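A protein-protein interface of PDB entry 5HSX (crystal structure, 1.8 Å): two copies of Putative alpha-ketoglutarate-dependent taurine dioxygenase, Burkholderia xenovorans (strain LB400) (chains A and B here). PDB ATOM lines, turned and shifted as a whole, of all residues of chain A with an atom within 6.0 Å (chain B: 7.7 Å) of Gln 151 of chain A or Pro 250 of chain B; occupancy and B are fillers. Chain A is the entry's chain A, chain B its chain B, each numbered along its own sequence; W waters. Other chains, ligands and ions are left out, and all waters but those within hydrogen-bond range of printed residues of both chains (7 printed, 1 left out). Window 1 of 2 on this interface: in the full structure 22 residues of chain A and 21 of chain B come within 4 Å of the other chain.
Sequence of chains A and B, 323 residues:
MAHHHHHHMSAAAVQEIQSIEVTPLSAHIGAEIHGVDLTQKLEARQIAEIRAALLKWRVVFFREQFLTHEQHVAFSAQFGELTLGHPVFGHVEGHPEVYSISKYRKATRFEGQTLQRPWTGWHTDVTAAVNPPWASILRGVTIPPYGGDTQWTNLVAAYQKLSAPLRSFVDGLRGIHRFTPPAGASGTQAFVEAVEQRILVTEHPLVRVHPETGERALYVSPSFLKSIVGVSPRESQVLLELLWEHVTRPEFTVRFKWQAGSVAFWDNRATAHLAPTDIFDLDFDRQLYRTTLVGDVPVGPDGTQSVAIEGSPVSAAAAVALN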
ATOM      1  N   PRO A 118     -25.090   9.609 -20.089  1.00  0.00           N
ATOM      2  CA  PRO A 118     -26.076   8.908 -20.933  1.00  0.00           C
ATOM      3  C   PRO A 118     -27.058   9.830 -21.620  1.00  0.00           C
ATOM      4  O   PRO A 118     -27.567   9.481 -22.691  1.00  0.00           O
ATOM      5  CB  PRO A 118     -26.795   7.986 -19.939  1.00  0.00           C
ATOM      6  CG  PRO A 118     -25.735   7.699 -18.900  1.00  0.00           C
ATOM      7  CD  PRO A 118     -24.973   8.989 -18.751  1.00  0.00           C
ATOM      8  N   TRP A 122     -29.369  14.426 -25.904  1.00  0.00           N
ATOM      9  CA  TRP A 122     -30.806  14.182 -25.971  1.00  0.00           C
ATOM     10  C   TRP A 122     -31.573  15.470 -25.723  1.00  0.00           C
ATOM     11  O   TRP A 122     -31.281  16.191 -24.766  1.00  0.00           O
ATOM     12  CB  TRP A 122     -31.221  13.138 -24.939  1.00  0.00           C
ATOM     13  CG  TRP A 122     -30.848  11.735 -25.331  1.00  0.00           C
ATOM     14  CD1 TRP A 122     -29.693  11.065 -25.015  1.00  0.00           C
ATOM     15  CD2 TRP A 122     -31.629  10.841 -26.137  1.00  0.00           C
ATOM     16  NE1 TRP A 122     -29.726   9.794 -25.558  1.00  0.00           N
ATOM     17  CE2 TRP A 122     -30.906   9.634 -26.247  1.00  0.00           C
ATOM     18  CE3 TRP A 122     -32.873  10.949 -26.781  1.00  0.00           C
ATOM     19  CZ2 TRP A 122     -31.387   8.537 -26.973  1.00  0.00           C
ATOM     20  CZ3 TRP A 122     -33.353   9.860 -27.498  1.00  0.00           C
ATOM     21  CH2 TRP A 122     -32.612   8.667 -27.586  1.00  0.00           C
ATOM     22  N   ASP A 149     -26.857   7.680 -37.720  1.00  0.00           N
ATOM     23  CA  ASP A 149     -28.193   7.301 -37.274  1.00  0.00           C
ATOM     24  C   ASP A 149     -28.739   8.306 -36.266  1.00  0.00           C
ATOM     25  O   ASP A 149     -27.988   8.947 -35.522  1.00  0.00           O
ATOM     26  CB  ASP A 149     -28.175   5.925 -36.598  1.00  0.00           C
ATOM     27  CG  ASP A 149     -27.856   4.793 -37.547  1.00  0.00           C
ATOM     28  OD1 ASP A 149     -27.585   5.042 -38.748  1.00  0.00           O
ATOM     29  OD2 ASP A 149     -27.855   3.639 -37.064  1.00  0.00           O
ATOM     30  N   THR A 150     -30.070   8.397 -36.209  1.00  0.00           N
ATOM     31  CA  THR A 150     -30.776   9.229 -35.242  1.00  0.00           C
ATOM     32  C   THR A 150     -31.592   8.340 -34.307  1.00  0.00           C
ATOM     33  O   THR A 150     -32.061   7.269 -34.705  1.00  0.00           O
ATOM     34  CB  THR A 150     -31.699  10.243 -35.959  1.00  0.00           C
ATOM     35  OG1 THR A 150     -30.920  10.989 -36.908  1.00  0.00           O
ATOM     36  CG2 THR A 150     -32.321  11.218 -34.960  1.00  0.00           C
ATOM     37  N   GLN A 151     -31.743   8.772 -33.048  1.00  0.00           N
ATOM     38  CA  GLN A 151     -32.560   8.032 -32.089  1.00  0.00           C
ATOM     39  C   GLN A 151     -33.623   8.936 -31.481  1.00  0.00           C
ATOM     40  O   GLN A 151     -33.428  10.144 -31.348  1.00  0.00           O
ATOM     41  CB  GLN A 151     -31.731   7.426 -30.964  1.00  0.00           C
ATOM     42  CG  GLN A 151     -30.571   6.553 -31.469  1.00  0.00           C
ATOM     43  CD  GLN A 151     -30.005   5.686 -30.378  1.00  0.00           C
ATOM     44  OE1 GLN A 151     -30.743   5.096 -29.587  1.00  0.00           O
ATOM     45  NE2 GLN A 151     -28.687   5.609 -30.317  1.00  0.00           N
ATOM     46  N   TRP A 152     -34.740   8.324 -31.096  1.00  0.00           N
ATOM     47  CA  TRP A 152     -35.832   8.998 -30.403  1.00  0.00           C
ATOM     48  C   TRP A 152     -36.179   8.209 -29.154  1.00  0.00           C
ATOM     49  O   TRP A 152     -36.000   6.990 -29.111  1.00  0.00           O
ATOM     50  CB  TRP A 152     -37.095   9.109 -31.282  1.00  0.00           C
ATOM     51  CG  TRP A 152     -37.003  10.101 -32.392  1.00  0.00           C
ATOM     52  CD1 TRP A 152     -37.539  11.358 -32.412  1.00  0.00           C
ATOM     53  CD2 TRP A 152     -36.351   9.921 -33.656  1.00  0.00           C
ATOM     54  NE1 TRP A 152     -37.254  11.972 -33.608  1.00  0.00           N
ATOM     55  CE2 TRP A 152     -36.522  11.112 -34.387  1.00  0.00           C
ATOM     56  CE3 TRP A 152     -35.640   8.866 -34.237  1.00  0.00           C
ATOM     57  CZ2 TRP A 152     -36.016  11.280 -35.670  1.00  0.00           C
ATOM     58  CZ3 TRP A 152     -35.129   9.034 -35.518  1.00  0.00           C
ATOM     59  CH2 TRP A 152     -35.324  10.228 -36.216  1.00  0.00           C
ATOM     60  N   THR A 153     -36.721   8.901 -28.148  1.00  0.00           N
ATOM     61  CA  THR A 153     -37.185   8.229 -26.947  1.00  0.00           C
ATOM     62  C   THR A 153     -38.611   8.667 -26.652  1.00  0.00           C
ATOM     63  O   THR A 153     -39.018   9.789 -26.972  1.00  0.00           O
ATOM     64  CB  THR A 153     -36.260   8.495 -25.740  1.00  0.00           C
ATOM     65  OG1 THR A 153     -36.698   7.697 -24.634  1.00  0.00           O
ATOM     66  CG2 THR A 153     -36.257   9.982 -25.340  1.00  0.00           C
ATOM     67  N   THR A 253     -36.554   3.616 -26.523  1.00  0.00           N
ATOM     68  CA  THR A 253     -35.948   4.258 -27.684  1.00  0.00           C
ATOM     69  C   THR A 253     -36.162   3.475 -28.976  1.00  0.00           C
ATOM     70  O   THR A 253     -36.486   2.282 -28.978  1.00  0.00           O
ATOM     71  CB  THR A 253     -34.437   4.460 -27.489  1.00  0.00           C
ATOM     72  OG1 THR A 253     -33.776   3.194 -27.512  1.00  0.00           O
ATOM     73  CG2 THR A 253     -34.161   5.149 -26.158  1.00  0.00           C
ATOM     74  N   VAL A 254     -35.959   4.183 -30.086  1.00  0.00           N
ATOM     75  CA  VAL A 254     -35.867   3.582 -31.410  1.00  0.00           C
ATOM     76  C   VAL A 254     -34.714   4.255 -32.143  1.00  0.00           C
ATOM     77  O   VAL A 254     -34.459   5.448 -31.958  1.00  0.00           O
ATOM     78  CB  VAL A 254     -37.187   3.710 -32.203  1.00  0.00           C
ATOM     79  CG1 VAL A 254     -37.509   5.180 -32.555  1.00  0.00           C
ATOM     80  CG2 VAL A 254     -37.145   2.854 -33.470  1.00  0.00           C
ATOM     81  N   ARG A 255     -34.007   3.480 -32.958  1.00  0.00           N
ATOM     82  CA  ARG A 255     -32.896   3.976 -33.756  1.00  0.00           C
ATOM     83  C   ARG A 255     -33.251   3.860 -35.234  1.00  0.00           C
ATOM     84  O   ARG A 255     -33.866   2.876 -35.660  1.00  0.00           O
ATOM     85  CB  ARG A 255     -31.621   3.196 -33.417  1.00  0.00           C
ATOM     86  CG  ARG A 255     -30.359   3.646 -34.152  1.00  0.00           C
ATOM     87  CD  ARG A 255     -29.138   3.029 -33.474  1.00  0.00           C
ATOM     88  NE  ARG A 255     -27.916   3.244 -34.247  1.00  0.00           N
ATOM     89  CZ  ARG A 255     -26.703   2.947 -33.803  1.00  0.00           C
ATOM     90  NH1 ARG A 255     -26.555   2.430 -32.589  1.00  0.00           N
ATOM     91  NH2 ARG A 255     -25.640   3.174 -34.567  1.00  0.00           N
ATOM     92  N   PHE A 256     -32.874   4.874 -36.014  1.00  0.00           N
ATOM     93  CA  PHE A 256     -33.206   4.951 -37.433  1.00  0.00           C
ATOM     94  C   PHE A 256     -31.929   5.140 -38.240  1.00  0.00           C
ATOM     95  O   PHE A 256     -31.171   6.085 -37.990  1.00  0.00           O
ATOM     96  CB  PHE A 256     -34.178   6.111 -37.677  1.00  0.00           C
ATOM     97  CG  PHE A 256     -34.714   6.196 -39.084  1.00  0.00           C
ATOM     98  CD1 PHE A 256     -35.613   5.250 -39.556  1.00  0.00           C
ATOM     99  CD2 PHE A 256     -34.365   7.257 -39.913  1.00  0.00           C
ATOM    100  CE1 PHE A 256     -36.148   5.350 -40.846  1.00  0.00           C
ATOM    101  CE2 PHE A 256     -34.892   7.361 -41.201  1.00  0.00           C
ATOM    102  CZ  PHE A 256     -35.784   6.403 -41.666  1.00  0.00           C
ATOM    103  N   ALA A 272     -38.037  12.965 -27.095  1.00  0.00           N
ATOM    104  CA  ALA A 272     -36.767  13.640 -27.255  1.00  0.00           C
ATOM    105  C   ALA A 272     -35.966  12.838 -28.270  1.00  0.00           C
ATOM    106  O   ALA A 272     -36.294  11.684 -28.576  1.00  0.00           O
ATOM    107  CB  ALA A 272     -36.008  13.772 -25.927  1.00  0.00           C
ATOM    108  N   HIS A 273     -34.945  13.459 -28.842  1.00  0.00           N
ATOM    109  CA  HIS A 273     -34.159  12.735 -29.825  1.00  0.00           C
ATOM    110  C   HIS A 273     -32.682  13.070 -29.696  1.00  0.00           C
ATOM    111  O   HIS A 273     -32.273  13.978 -28.972  1.00  0.00           O
ATOM    112  CB  HIS A 273     -34.653  13.000 -31.255  1.00  0.00           C
ATOM    113  CG  HIS A 273     -34.682  14.445 -31.640  1.00  0.00           C
ATOM    114  ND1 HIS A 273     -33.711  15.022 -32.432  1.00  0.00           N
ATOM    115  CD2 HIS A 273     -35.580  15.422 -31.370  1.00  0.00           C
ATOM    116  CE1 HIS A 273     -34.004  16.297 -32.625  1.00  0.00           C
ATOM    117  NE2 HIS A 273     -35.132  16.565 -31.991  1.00  0.00           N
ATOM    118  N   LEU A 274     -31.883  12.314 -30.441  1.00  0.00           N
ATOM    119  CA  LEU A 274     -30.442  12.317 -30.283  1.00  0.00           C
ATOM    120  C   LEU A 274     -29.793  12.318 -31.658  1.00  0.00           C
ATOM    121  O   LEU A 274     -29.969  11.370 -32.429  1.00  0.00           O
ATOM    122  CB  LEU A 274     -29.998  11.082 -29.488  1.00  0.00           C
ATOM    123  CG  LEU A 274     -28.484  10.888 -29.439  1.00  0.00           C
ATOM    124  CD1 LEU A 274     -27.801  12.022 -28.648  1.00  0.00           C
ATOM    125  CD2 LEU A 274     -28.169   9.501 -28.851  1.00  0.00           C
ATOM    126  N   ALA A 275     -29.046  13.384 -31.958  1.00  0.00           N
ATOM    127  CA  ALA A 275     -28.345  13.461 -33.229  1.00  0.00           C
ATOM    128  C   ALA A 275     -27.062  12.633 -33.170  1.00  0.00           C
ATOM    129  O   ALA A 275     -26.510  12.406 -32.092  1.00  0.00           O
ATOM    130  CB  ALA A 275     -28.011  14.913 -33.566  1.00  0.00           C
ATOM    131  N   SER B  26     -22.617   0.917 -38.921  1.00  0.00           N
ATOM    132  CA  SER B  26     -22.325   2.110 -38.135  1.00  0.00           C
ATOM    133  C   SER B  26     -20.859   2.439 -38.360  1.00  0.00           C
ATOM    134  O   SER B  26     -20.163   1.732 -39.088  1.00  0.00           O
ATOM    135  CB  SER B  26     -22.636   1.908 -36.648  1.00  0.00           C
ATOM    136  OG  SER B  26     -21.648   1.098 -36.027  1.00  0.00           O
ATOM    137  N   ILE B  29     -18.959  -0.496 -35.803  1.00  0.00           N
ATOM    138  CA  ILE B  29     -19.376  -1.842 -35.410  1.00  0.00           C
ATOM    139  C   ILE B  29     -20.593  -2.281 -36.212  1.00  0.00           C
ATOM    140  O   ILE B  29     -21.550  -1.524 -36.406  1.00  0.00           O
ATOM    141  CB  ILE B  29     -19.633  -1.938 -33.887  1.00  0.00           C
ATOM    142  CG1 ILE B  29     -20.001  -3.372 -33.508  1.00  0.00           C
ATOM    143  CG2 ILE B  29     -20.716  -0.936 -33.428  1.00  0.00           C
ATOM    144  CD1 ILE B  29     -19.968  -3.624 -32.011  1.00  0.00           C
ATOM    145  N   GLN B 151     -28.495  -5.413 -29.141  1.00  0.00           N
ATOM    146  CA  GLN B 151     -27.455  -4.418 -29.357  1.00  0.00           C
ATOM    147  C   GLN B 151     -26.093  -4.982 -28.982  1.00  0.00           C
ATOM    148  O   GLN B 151     -25.971  -5.839 -28.101  1.00  0.00           O
ATOM    149  CB  GLN B 151     -27.698  -3.135 -28.555  1.00  0.00           C
ATOM    150  CG  GLN B 151     -29.091  -2.525 -28.763  1.00  0.00           C
ATOM    151  CD  GLN B 151     -29.172  -1.097 -28.274  1.00  0.00           C
ATOM    152  OE1 GLN B 151     -28.286  -0.291 -28.544  1.00  0.00           O
ATOM    153  NE2 GLN B 151     -30.254  -0.768 -27.557  1.00  0.00           N
ATOM    154  N   TRP B 152     -25.066  -4.466 -29.654  1.00  0.00           N
ATOM    155  CA  TRP B 152     -23.678  -4.781 -29.354  1.00  0.00           C
ATOM    156  C   TRP B 152     -22.892  -3.488 -29.176  1.00  0.00           C
ATOM    157  O   TRP B 152     -23.227  -2.453 -29.761  1.00  0.00           O
ATOM    158  CB  TRP B 152     -23.009  -5.611 -30.482  1.00  0.00           C
ATOM    159  CG  TRP B 152     -23.458  -7.049 -30.579  1.00  0.00           C
ATOM    160  CD1 TRP B 152     -22.776  -8.156 -30.143  1.00  0.00           C
ATOM    161  CD2 TRP B 152     -24.667  -7.529 -31.171  1.00  0.00           C
ATOM    162  NE1 TRP B 152     -23.498  -9.294 -30.416  1.00  0.00           N
ATOM    163  CE2 TRP B 152     -24.662  -8.937 -31.049  1.00  0.00           C
ATOM    164  CE3 TRP B 152     -25.754  -6.909 -31.794  1.00  0.00           C
ATOM    165  CZ2 TRP B 152     -25.706  -9.733 -31.529  1.00  0.00           C
ATOM    166  CZ3 TRP B 152     -26.799  -7.706 -32.263  1.00  0.00           C
ATOM    167  CH2 TRP B 152     -26.761  -9.097 -32.131  1.00  0.00           C
ATOM    168  N   THR B 153     -21.813  -3.558 -28.402  1.00  0.00           N
ATOM    169  CA  THR B 153     -20.923  -2.418 -28.281  1.00  0.00           C
ATOM    170  C   THR B 153     -19.490  -2.862 -28.537  1.00  0.00           C
ATOM    171  O   THR B 153     -19.122  -4.006 -28.270  1.00  0.00           O
ATOM    172  CB  THR B 153     -21.052  -1.743 -26.923  1.00  0.00           C
ATOM    173  OG1 THR B 153     -20.232  -0.569 -26.913  1.00  0.00           O
ATOM    174  CG2 THR B 153     -20.649  -2.705 -25.775  1.00  0.00           C
ATOM    175  N   GLU B 245     -20.350   3.209 -17.878  1.00  0.00           N
ATOM    176  CA  GLU B 245     -21.015   4.308 -18.570  1.00  0.00           C
ATOM    177  C   GLU B 245     -20.342   4.577 -19.914  1.00  0.00           C
ATOM    178  O   GLU B 245     -21.009   4.786 -20.938  1.00  0.00           O
ATOM    179  CB  GLU B 245     -20.982   5.533 -17.658  1.00  0.00           C
ATOM    180  CG  GLU B 245     -21.182   6.876 -18.289  1.00  0.00           C
ATOM    181  CD  GLU B 245     -21.125   7.977 -17.239  1.00  0.00           C
ATOM    182  OE1 GLU B 245     -22.210   8.418 -16.848  1.00  0.00           O
ATOM    183  OE2 GLU B 245     -20.010   8.355 -16.763  1.00  0.00           O
ATOM    184  N   HIS B 246     -19.014   4.533 -19.928  1.00  0.00           N
ATOM    185  CA  HIS B 246     -18.262   4.807 -21.146  1.00  0.00           C
ATOM    186  C   HIS B 246     -18.593   3.794 -22.245  1.00  0.00           C
ATOM    187  O   HIS B 246     -18.857   4.175 -23.393  1.00  0.00           O
ATOM    188  CB  HIS B 246     -16.769   4.803 -20.797  1.00  0.00           C
ATOM    189  CG  HIS B 246     -15.855   5.047 -21.963  1.00  0.00           C
ATOM    190  ND1 HIS B 246     -15.669   6.293 -22.518  1.00  0.00           N
ATOM    191  CD2 HIS B 246     -15.057   4.198 -22.657  1.00  0.00           C
ATOM    192  CE1 HIS B 246     -14.793   6.206 -23.509  1.00  0.00           C
ATOM    193  NE2 HIS B 246     -14.411   4.946 -23.616  1.00  0.00           N
ATOM    194  N   VAL B 247     -18.586   2.495 -21.921  1.00  0.00           N
ATOM    195  CA  VAL B 247     -18.724   1.482 -22.969  1.00  0.00           C
ATOM    196  C   VAL B 247     -20.124   1.420 -23.540  1.00  0.00           C
ATOM    197  O   VAL B 247     -20.320   0.795 -24.586  1.00  0.00           O
ATOM    198  CB  VAL B 247     -18.365   0.043 -22.524  1.00  0.00           C
ATOM    199  CG1 VAL B 247     -16.920  -0.045 -22.084  1.00  0.00           C
ATOM    200  CG2 VAL B 247     -19.345  -0.491 -21.459  1.00  0.00           C
ATOM    201  N   THR B 248     -21.104   2.034 -22.881  1.00  0.00           N
ATOM    202  CA  THR B 248     -22.455   2.045 -23.400  1.00  0.00           C
ATOM    203  C   THR B 248     -22.785   3.333 -24.141  1.00  0.00           C
ATOM    204  O   THR B 248     -23.954   3.549 -24.479  1.00  0.00           O
ATOM    205  CB  THR B 248     -23.476   1.787 -22.268  1.00  0.00           C
ATOM    206  OG1 THR B 248     -23.240   2.663 -21.161  1.00  0.00           O
ATOM    207  CG2 THR B 248     -23.357   0.348 -21.781  1.00  0.00           C
ATOM    208  N   ARG B 249     -21.793   4.177 -24.434  1.00  0.00           N
ATOM    209  CA  ARG B 249     -22.083   5.379 -25.212  1.00  0.00           C
ATOM    210  C   ARG B 249     -22.540   4.992 -26.619  1.00  0.00           C
ATOM    211  O   ARG B 249     -22.005   4.044 -27.207  1.00  0.00           O
ATOM    212  CB  ARG B 249     -20.867   6.311 -25.267  1.00  0.00           C
ATOM    213  CG  ARG B 249     -20.658   7.008 -23.911  1.00  0.00           C
ATOM    214  CD  ARG B 249     -20.242   8.456 -24.040  1.00  0.00           C
ATOM    215  NE  ARG B 249     -18.954   8.600 -24.712  1.00  0.00           N
ATOM    216  CZ  ARG B 249     -17.769   8.553 -24.104  1.00  0.00           C
ATOM    217  NH1 ARG B 249     -16.667   8.708 -24.833  1.00  0.00           N
ATOM    218  NH2 ARG B 249     -17.677   8.348 -22.778  1.00  0.00           N
ATOM    219  N   PRO B 250     -23.559   5.677 -27.163  1.00  0.00           N
ATOM    220  CA  PRO B 250     -24.143   5.271 -28.458  1.00  0.00           C
ATOM    221  C   PRO B 250     -23.148   5.187 -29.595  1.00  0.00           C
ATOM    222  O   PRO B 250     -23.348   4.388 -30.519  1.00  0.00           O
ATOM    223  CB  PRO B 250     -25.194   6.366 -28.724  1.00  0.00           C
ATOM    224  CG  PRO B 250     -25.530   6.912 -27.386  1.00  0.00           C
ATOM    225  CD  PRO B 250     -24.281   6.804 -26.547  1.00  0.00           C
ATOM    226  N   GLU B 251     -22.086   5.992 -29.565  1.00  0.00           N
ATOM    227  CA  GLU B 251     -21.108   5.960 -30.647  1.00  0.00           C
ATOM    228  C   GLU B 251     -20.407   4.612 -30.766  1.00  0.00           C
ATOM    229  O   GLU B 251     -19.820   4.327 -31.818  1.00  0.00           O
ATOM    230  CB  GLU B 251     -20.068   7.056 -30.439  1.00  0.00           C
ATOM    231  CG  GLU B 251     -19.096   6.746 -29.317  1.00  0.00           C
ATOM    232  CD  GLU B 251     -18.441   7.986 -28.735  1.00  0.00           C
ATOM    233  OE1 GLU B 251     -19.072   8.639 -27.872  1.00  0.00           O
ATOM    234  OE2 GLU B 251     -17.298   8.306 -29.137  1.00  0.00           O
ATOM    235  N   PHE B 252     -20.435   3.781 -29.719  1.00  0.00           N
ATOM    236  CA  PHE B 252     -19.778   2.476 -29.765  1.00  0.00           C
ATOM    237  C   PHE B 252     -20.733   1.345 -30.129  1.00  0.00           C
ATOM    238  O   PHE B 252     -20.292   0.198 -30.207  1.00  0.00           O
ATOM    239  CB  PHE B 252     -19.112   2.139 -28.411  1.00  0.00           C
ATOM    240  CG  PHE B 252     -18.141   3.181 -27.926  1.00  0.00           C
ATOM    241  CD1 PHE B 252     -17.142   3.663 -28.767  1.00  0.00           C
ATOM    242  CD2 PHE B 252     -18.232   3.682 -26.631  1.00  0.00           C
ATOM    243  CE1 PHE B 252     -16.247   4.632 -28.324  1.00  0.00           C
ATOM    244  CE2 PHE B 252     -17.348   4.654 -26.179  1.00  0.00           C
ATOM    245  CZ  PHE B 252     -16.349   5.129 -27.032  1.00  0.00           C
ATOM    246  N   THR B 253     -22.017   1.628 -30.377  1.00  0.00           N
ATOM    247  CA  THR B 253     -23.026   0.575 -30.422  1.00  0.00           C
ATOM    248  C   THR B 253     -23.649   0.403 -31.803  1.00  0.00           C
ATOM    249  O   THR B 253     -23.614   1.295 -32.653  1.00  0.00           O
ATOM    250  CB  THR B 253     -24.170   0.825 -29.415  1.00  0.00           C
ATOM    251  OG1 THR B 253     -24.973   1.935 -29.851  1.00  0.00           O
ATOM    252  CG2 THR B 253     -23.610   1.088 -28.029  1.00  0.00           C
ATOM    253  N   VAL B 254     -24.242  -0.774 -32.000  1.00  0.00           N
ATOM    254  CA  VAL B 254     -25.117  -1.042 -33.139  1.00  0.00           C
ATOM    255  C   VAL B 254     -26.335  -1.809 -32.635  1.00  0.00           C
ATOM    256  O   VAL B 254     -26.231  -2.621 -31.711  1.00  0.00           O
ATOM    257  CB  VAL B 254     -24.378  -1.819 -34.259  1.00  0.00           C
ATOM    258  CG1 VAL B 254     -23.987  -3.239 -33.790  1.00  0.00           C
ATOM    259  CG2 VAL B 254     -25.229  -1.870 -35.529  1.00  0.00           C
ATOM    260  N   ARG B 255     -27.493  -1.533 -33.235  1.00  0.00           N
ATOM    261  CA  ARG B 255     -28.753  -2.186 -32.901  1.00  0.00           C
ATOM    262  C   ARG B 255     -29.227  -3.005 -34.095  1.00  0.00           C
ATOM    263  O   ARG B 255     -29.097  -2.570 -35.246  1.00  0.00           O
ATOM    264  CB  ARG B 255     -29.800  -1.134 -32.504  1.00  0.00           C
ATOM    265  CG  ARG B 255     -31.166  -1.685 -32.093  1.00  0.00           C
ATOM    266  CD  ARG B 255     -31.978  -0.566 -31.460  1.00  0.00           C
ATOM    267  NE  ARG B 255     -33.340  -0.988 -31.166  1.00  0.00           N
ATOM    268  CZ  ARG B 255     -34.170  -0.307 -30.380  1.00  0.00           C
ATOM    269  NH1 ARG B 255     -33.757   0.807 -29.795  1.00  0.00           N
ATOM    270  NH2 ARG B 255     -35.412  -0.755 -30.170  1.00  0.00           N
HETATM  271  O   HOH W   1     -27.137   3.389 -28.715  1.00  0.00           O
HETATM  272  O   HOH W   2     -31.169   2.327 -29.801  1.00  0.00           O
HETATM  273  O   HOH W   3     -30.920   2.281 -27.004  1.00  0.00           O
HETATM  274  O   HOH W   4     -37.140   0.037 -27.755  1.00  0.00           O
HETATM  275  O   HOH W   5     -34.167   0.789 -33.766  1.00  0.00           O
HETATM  276  O   HOH W   6     -28.260   0.193 -35.447  1.00  0.00           O
HETATM  277  O   HOH W   7     -28.534   1.716 -30.402  1.00  0.00           O
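The guanidinium group (NH1) of Arg 255 of chain B lies within hydrogen-bond range of the backbone carbonyl oxygen (O) of Thr 253 of chain A, 3.2 Å away.
NH1 of Arg 255 of chain A is in hydrogen-bond range of O of Thr 253 of chain B, 3.2 Å away.
The side-chain carboxylate of Asp 149 of chain A is in salt-bridge range of the guanidinium group of Arg 255 of chain A.
The backbone NH (N) of Leu 274 of chain A lies within hydrogen-bond range of the backbone carbonyl oxygen (O) of Gln 151 of chain A, 2.8 Å away.
The side-chain hydroxyl of Ser 26 of chain B sits at hydrogen-bond distance from the backbone carbonyl oxygen of Ile 29 of chain B, 2.7 Å away.
The backbone NH (N) of Val 254 of chain B lies within hydrogen-bond range of the backbone carbonyl oxygen (O) of Trp 152 of chain B (3.0 Å).
The backbone carbonyl oxygen of Glu 245 of chain B is in hydrogen-bond range of the side-chain hydroxyl of Thr 248 of chain B (3.1 Å).
The backbone carbonyl oxygen of Pro 250 of chain B is in hydrogen-bond range of the side-chain hydroxyl of Thr 253 of chain B, at 3.0 Å.
Pro 118 of chain A touches Glu 245 of chain B (CD to OE1, 3.4 Å).
Gln 151 of chain A touches Pro 250 of chain B (NE2 to CB, 3.9 Å).
Arg 255 of chain B touches Val 254 of chain A (NH1 to CA, 3.8 Å).
CB of Ser 26 of chain B touches NH2 of Arg 255 of chain A (3.9 Å).
Arg 255 of chain A touches Val 254 of chain B (NH1 to CA, 3.8 Å).
Leu 274 of chain A touches Pro 250 of chain B (CD2 to CG, 3.98 Å).
Pro 250 of chain B touches just these residues of chain A: Gln 151 and Leu 274.
Of the printed residues of chain A, Thr 253 of chain B touches Arg 255 (3.2 Å).
Printed residues of chain B within 4 Å of Val 254 of chain A: Arg 255.
Glu 251 of chain B touches none of the printed residues of chain A.
Phe 252 of chain B touches none of the printed residues of chain A.
The nearest residue of chain A that does not touch Pro 250 of chain B is Arg 255 of chain A (4.3 Å).
The nearest printed residue of chain A that does not touch Thr 253 of chain B is Gln 151 of chain A (5.2 Å).
Printed residues of chain B that touch a printed residue of chain A: Ser 26, Glu 245, Pro 250, Thr 253, Val 254 and Arg 255.
Hydrophobic or aromatic side chains of chain B within 4 Å of the printed part of chain A: Pro 250.
Of the 15 printed residues of chain A, 6 touch a printed residue of chain B.
Hydrophobic or aromatic side chains of chain A within 4 Å of the printed part of chain B: Pro 118 and Leu 274.
Thr 253 of chain A touches Arg 255 of chain B, and with the chains exchanged Arg 255 of chain A touches Thr 253 of chain B.
Val 254 of chain A touches Arg 255 of chain B, and with the chains exchanged Arg 255 of chain A touches Val 254 of chain B.
Positions printed for both chains: 151, 152, 153, 253, 254 and 255.
Of the 8 pairs that touch across the chains among the printed residues, 4 have their exchanged pair printed and touching as well.
Water W4 bridges O of Thr 253 of chain A (2.6 Å) and NH2 of Arg 255 of chain B (3.1 Å).
Water W7 bridges OE1 of Gln 151 of chain B (2.7 Å) and NH1 of Arg 255 of chain A (3.0 Å).
Water W2 bridges the side-chain amide oxygen of Gln 151 of chain A (2.8 Å) and the guanidinium group of Arg 255 of chain B (3.0 Å).
Water W5 lies within hydrogen-bond range of N of Arg 255 of chain A (2.8 Å) and NE of Arg 255 of chain B (3.3 Å).
Water W1 bridges the side-chain hydroxyl of Thr 253 of chain B and the side-chain amide nitrogen of Gln 151 of chain A.
Water W6 bridges O of Arg 255 of chain B (2.9 Å) and NE of Arg 255 of chain A (3.3 Å).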
